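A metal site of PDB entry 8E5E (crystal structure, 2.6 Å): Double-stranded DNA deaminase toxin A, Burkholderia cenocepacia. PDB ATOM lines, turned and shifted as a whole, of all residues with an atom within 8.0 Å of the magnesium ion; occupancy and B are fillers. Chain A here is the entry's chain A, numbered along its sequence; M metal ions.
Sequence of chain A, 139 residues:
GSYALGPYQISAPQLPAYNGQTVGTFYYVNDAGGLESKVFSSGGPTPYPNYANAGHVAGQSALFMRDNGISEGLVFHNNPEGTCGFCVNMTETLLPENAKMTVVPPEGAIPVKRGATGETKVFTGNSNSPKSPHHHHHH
The side-chain carboxylate (OE2) of Glu 92 lies within hydrogen-bond range of the backbone NH (N) of Thr 124. O of Leu 95 lies close to NH2 of Arg 66 (3.5 Å).
Of the 18 residues printed, 5 come within 4 Å of the magnesium ion.
The magnesium ion is bound by OD1 of Asn 126. The magnesium ion is bound by the backbone carbonyl oxygen (O) of Asn 128 (2.2 Å). O of Glu 92 binds the magnesium ion (2.2 Å). O of Asn 126 binds the magnesium ion, at 2.3 Å. The backbone carbonyl oxygen (O) of Thr 93 binds the magnesium ion (2.3 Å). The backbone carbonyl oxygen (O) of Leu 95 binds the magnesium ion (2.5 Å). The magnesium ion has six donor atoms within binding distance.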
ATOM      1  N   ARG A  66      21.456   8.574 -12.383  1.00  0.00           N
ATOM      2  CA  ARG A  66      20.545   7.797 -11.543  1.00  0.00           C
ATOM      3  C   ARG A  66      19.104   8.227 -11.738  1.00  0.00           C
ATOM      4  O   ARG A  66      18.194   7.397 -11.819  1.00  0.00           O
ATOM      5  CB  ARG A  66      20.955   7.930 -10.076  1.00  0.00           C
ATOM      6  CG  ARG A  66      19.924   7.390  -9.091  1.00  0.00           C
ATOM      7  CD  ARG A  66      20.404   7.523  -7.646  1.00  0.00           C
ATOM      8  NE  ARG A  66      21.462   6.563  -7.333  1.00  0.00           N
ATOM      9  CZ  ARG A  66      21.272   5.398  -6.731  1.00  0.00           C
ATOM     10  NH1 ARG A  66      20.059   5.016  -6.341  1.00  0.00           N
ATOM     11  NH2 ARG A  66      22.302   4.596  -6.505  1.00  0.00           N
ATOM     12  N   MET A  90      33.200   7.671  -3.572  1.00  0.00           N
ATOM     13  CA  MET A  90      31.769   7.698  -3.319  1.00  0.00           C
ATOM     14  C   MET A  90      30.914   7.757  -4.593  1.00  0.00           C
ATOM     15  O   MET A  90      29.681   7.639  -4.497  1.00  0.00           O
ATOM     16  CB  MET A  90      31.419   8.894  -2.419  1.00  0.00           C
ATOM     17  CG  MET A  90      32.522   9.199  -1.407  1.00  0.00           C
ATOM     18  SD  MET A  90      32.120  10.470  -0.194  1.00  0.00           S
ATOM     19  CE  MET A  90      30.941   9.588   0.819  1.00  0.00           C
ATOM     20  N   THR A  91      31.532   7.918  -5.761  1.00  0.00           N
ATOM     21  CA  THR A  91      30.769   7.998  -7.001  1.00  0.00           C
ATOM     22  C   THR A  91      30.031   6.696  -7.287  1.00  0.00           C
ATOM     23  O   THR A  91      28.835   6.691  -7.596  1.00  0.00           O
ATOM     24  CB  THR A  91      31.695   8.361  -8.169  1.00  0.00           C
ATOM     25  OG1 THR A  91      32.175   9.698  -7.997  1.00  0.00           O
ATOM     26  CG2 THR A  91      30.956   8.244  -9.499  1.00  0.00           C
ATOM     27  N   GLU A  92      30.743   5.561  -7.194  1.00  0.00           N
ATOM     28  CA  GLU A  92      30.116   4.271  -7.435  1.00  0.00           C
ATOM     29  C   GLU A  92      28.977   4.013  -6.470  1.00  0.00           C
ATOM     30  O   GLU A  92      27.980   3.365  -6.824  1.00  0.00           O
ATOM     31  CB  GLU A  92      31.160   3.156  -7.365  1.00  0.00           C
ATOM     32  CG  GLU A  92      32.268   3.277  -8.402  1.00  0.00           C
ATOM     33  CD  GLU A  92      33.238   2.117  -8.371  1.00  0.00           C
ATOM     34  OE1 GLU A  92      33.362   1.461  -7.315  1.00  0.00           O
ATOM     35  OE2 GLU A  92      33.884   1.855  -9.403  1.00  0.00           O
ATOM     36  N   THR A  93      29.085   4.519  -5.232  1.00  0.00           N
ATOM     37  CA  THR A  93      27.944   4.502  -4.341  1.00  0.00           C
ATOM     38  C   THR A  93      26.791   5.289  -4.950  1.00  0.00           C
ATOM     39  O   THR A  93      25.702   4.740  -5.171  1.00  0.00           O
ATOM     40  CB  THR A  93      28.329   5.077  -2.972  1.00  0.00           C
ATOM     41  OG1 THR A  93      29.351   4.265  -2.384  1.00  0.00           O
ATOM     42  CG2 THR A  93      27.114   5.123  -2.052  1.00  0.00           C
ATOM     43  N   LEU A  94      27.022   6.570  -5.252  1.00  0.00           N
ATOM     44  CA  LEU A  94      25.984   7.418  -5.826  1.00  0.00           C
ATOM     45  C   LEU A  94      25.460   6.854  -7.144  1.00  0.00           C
ATOM     46  O   LEU A  94      24.250   6.929  -7.419  1.00  0.00           O
ATOM     47  CB  LEU A  94      26.509   8.841  -6.033  1.00  0.00           C
ATOM     48  CG  LEU A  94      26.922   9.658  -4.811  1.00  0.00           C
ATOM     49  CD1 LEU A  94      27.343  11.051  -5.234  1.00  0.00           C
ATOM     50  CD2 LEU A  94      25.798   9.709  -3.792  1.00  0.00           C
ATOM     51  N   LEU A  95      26.345   6.312  -7.966  1.00  0.00           N
ATOM     52  CA  LEU A  95      25.956   5.813  -9.270  1.00  0.00           C
ATOM     53  C   LEU A  95      25.027   4.604  -9.122  1.00  0.00           C
ATOM     54  O   LEU A  95      25.217   3.785  -8.216  1.00  0.00           O
ATOM     55  CB  LEU A  95      27.205   5.430 -10.075  1.00  0.00           C
ATOM     56  CG  LEU A  95      27.242   5.622 -11.584  1.00  0.00           C
ATOM     57  CD1 LEU A  95      26.655   6.955 -11.990  1.00  0.00           C
ATOM     58  CD2 LEU A  95      28.686   5.523 -12.067  1.00  0.00           C
ATOM     59  N   PRO A  96      24.009   4.483  -9.973  1.00  0.00           N
ATOM     60  CA  PRO A  96      23.160   3.282  -9.942  1.00  0.00           C
ATOM     61  C   PRO A  96      23.962   2.052 -10.332  1.00  0.00           C
ATOM     62  O   PRO A  96      25.028   2.129 -10.938  1.00  0.00           O
ATOM     63  CB  PRO A  96      22.065   3.581 -10.966  1.00  0.00           C
ATOM     64  CG  PRO A  96      22.656   4.628 -11.860  1.00  0.00           C
ATOM     65  CD  PRO A  96      23.550   5.453 -10.988  1.00  0.00           C
ATOM     66  N   GLU A  97      23.429   0.891  -9.968  1.00  0.00           N
ATOM     67  CA  GLU A  97      24.160  -0.362 -10.116  1.00  0.00           C
ATOM     68  C   GLU A  97      24.481  -0.634 -11.579  1.00  0.00           C
ATOM     69  O   GLU A  97      23.640  -0.438 -12.464  1.00  0.00           O
ATOM     70  CB  GLU A  97      23.368  -1.523  -9.521  1.00  0.00           C
ATOM     71  CG  GLU A  97      24.168  -2.807  -9.417  1.00  0.00           C
ATOM     72  CD  GLU A  97      23.400  -3.920  -8.741  1.00  0.00           C
ATOM     73  OE1 GLU A  97      22.152  -3.847  -8.718  1.00  0.00           O
ATOM     74  OE2 GLU A  97      24.039  -4.867  -8.248  1.00  0.00           O
ATOM     75  N   ASN A  98      25.720  -1.057 -11.832  1.00  0.00           N
ATOM     76  CA  ASN A  98      26.298  -1.395 -13.133  1.00  0.00           C
ATOM     77  C   ASN A  98      26.347  -0.219 -14.104  1.00  0.00           C
ATOM     78  O   ASN A  98      26.675  -0.428 -15.284  1.00  0.00           O
ATOM     79  CB  ASN A  98      25.568  -2.561 -13.819  1.00  0.00           C
ATOM     80  CG  ASN A  98      25.649  -3.850 -13.032  1.00  0.00           C
ATOM     81  OD1 ASN A  98      26.598  -4.086 -12.284  1.00  0.00           O
ATOM     82  ND2 ASN A  98      24.637  -4.701 -13.197  1.00  0.00           N
ATOM     83  N   ALA A  99      26.057   1.003 -13.662  1.00  0.00           N
ATOM     84  CA  ALA A  99      26.163   2.141 -14.554  1.00  0.00           C
ATOM     85  C   ALA A  99      27.627   2.512 -14.763  1.00  0.00           C
ATOM     86  O   ALA A  99      28.426   2.529 -13.812  1.00  0.00           O
ATOM     87  CB  ALA A  99      25.389   3.334 -14.002  1.00  0.00           C
ATOM     88  N   THR A 124      32.239   2.289 -11.983  1.00  0.00           N
ATOM     89  CA  THR A 124      31.185   1.302 -12.220  1.00  0.00           C
ATOM     90  C   THR A 124      30.297   1.282 -10.975  1.00  0.00           C
ATOM     91  O   THR A 124      30.745   0.912  -9.899  1.00  0.00           O
ATOM     92  CB  THR A 124      31.764  -0.082 -12.499  1.00  0.00           C
ATOM     93  OG1 THR A 124      32.616  -0.020 -13.660  1.00  0.00           O
ATOM     94  CG2 THR A 124      30.658  -1.099 -12.748  1.00  0.00           C
ATOM     95  N   GLY A 125      29.035   1.694 -11.140  1.00  0.00           N
ATOM     96  CA  GLY A 125      28.162   1.856  -9.997  1.00  0.00           C
ATOM     97  C   GLY A 125      27.929   0.535  -9.277  1.00  0.00           C
ATOM     98  O   GLY A 125      27.860  -0.534  -9.898  1.00  0.00           O
ATOM     99  N   ASN A 126      27.812   0.615  -7.960  1.00  0.00           N
ATOM    100  CA  ASN A 126      27.583  -0.544  -7.112  1.00  0.00           C
ATOM    101  C   ASN A 126      26.151  -0.555  -6.615  1.00  0.00           C
ATOM    102  O   ASN A 126      25.450   0.465  -6.621  1.00  0.00           O
ATOM    103  CB  ASN A 126      28.562  -0.562  -5.932  1.00  0.00           C
ATOM    104  CG  ASN A 126      28.393   0.642  -5.028  1.00  0.00           C
ATOM    105  OD1 ASN A 126      27.397   1.369  -5.115  1.00  0.00           O
ATOM    106  ND2 ASN A 126      29.357   0.849  -4.133  1.00  0.00           N
ATOM    107  N   SER A 127      25.728  -1.730  -6.138  1.00  0.00           N
ATOM    108  CA  SER A 127      24.339  -1.935  -5.711  1.00  0.00           C
ATOM    109  C   SER A 127      23.948  -1.007  -4.556  1.00  0.00           C
ATOM    110  O   SER A 127      22.756  -0.879  -4.269  1.00  0.00           O
ATOM    111  CB  SER A 127      24.124  -3.389  -5.300  1.00  0.00           C
ATOM    112  OG  SER A 127      24.925  -3.736  -4.185  1.00  0.00           O
ATOM    113  N   ASN A 128      24.916  -0.373  -3.910  1.00  0.00           N
ATOM    114  CA  ASN A 128      24.606   0.570  -2.843  1.00  0.00           C
ATOM    115  C   ASN A 128      24.045   1.861  -3.425  1.00  0.00           C
ATOM    116  O   ASN A 128      24.576   2.412  -4.400  1.00  0.00           O
ATOM    117  CB  ASN A 128      25.848   0.855  -2.003  1.00  0.00           C
ATOM    118  CG  ASN A 128      26.472  -0.402  -1.430  1.00  0.00           C
ATOM    119  OD1 ASN A 128      25.782  -1.394  -1.192  1.00  0.00           O
ATOM    120  ND2 ASN A 128      27.791  -0.367  -1.222  1.00  0.00           N
ATOM    121  N   SER A 129      22.964   2.352  -2.812  1.00  0.00           N
ATOM    122  CA  SER A 129      22.281   3.603  -3.065  1.00  0.00           C
ATOM    123  C   SER A 129      22.630   4.619  -1.988  1.00  0.00           C
ATOM    124  O   SER A 129      22.947   4.242  -0.856  1.00  0.00           O
ATOM    125  CB  SER A 129      20.758   3.386  -3.104  1.00  0.00           C
ATOM    126  OG  SER A 129      20.298   2.812  -1.889  1.00  0.00           O
ATOM    127  N   PRO A 130      22.591   5.910  -2.295  1.00  0.00           N
ATOM    128  CA  PRO A 130      22.989   6.923  -1.311  1.00  0.00           C
ATOM    129  C   PRO A 130      22.054   6.937  -0.113  1.00  0.00           C
ATOM    130  O   PRO A 130      20.838   6.797  -0.249  1.00  0.00           O
ATOM    131  CB  PRO A 130      22.920   8.232  -2.093  1.00  0.00           C
ATOM    132  CG  PRO A 130      21.979   7.963  -3.210  1.00  0.00           C
ATOM    133  CD  PRO A 130      22.202   6.526  -3.581  1.00  0.00           C
HETATM  134 MG    MG M   1      25.970   2.653  -6.127  1.00  0.00          MG
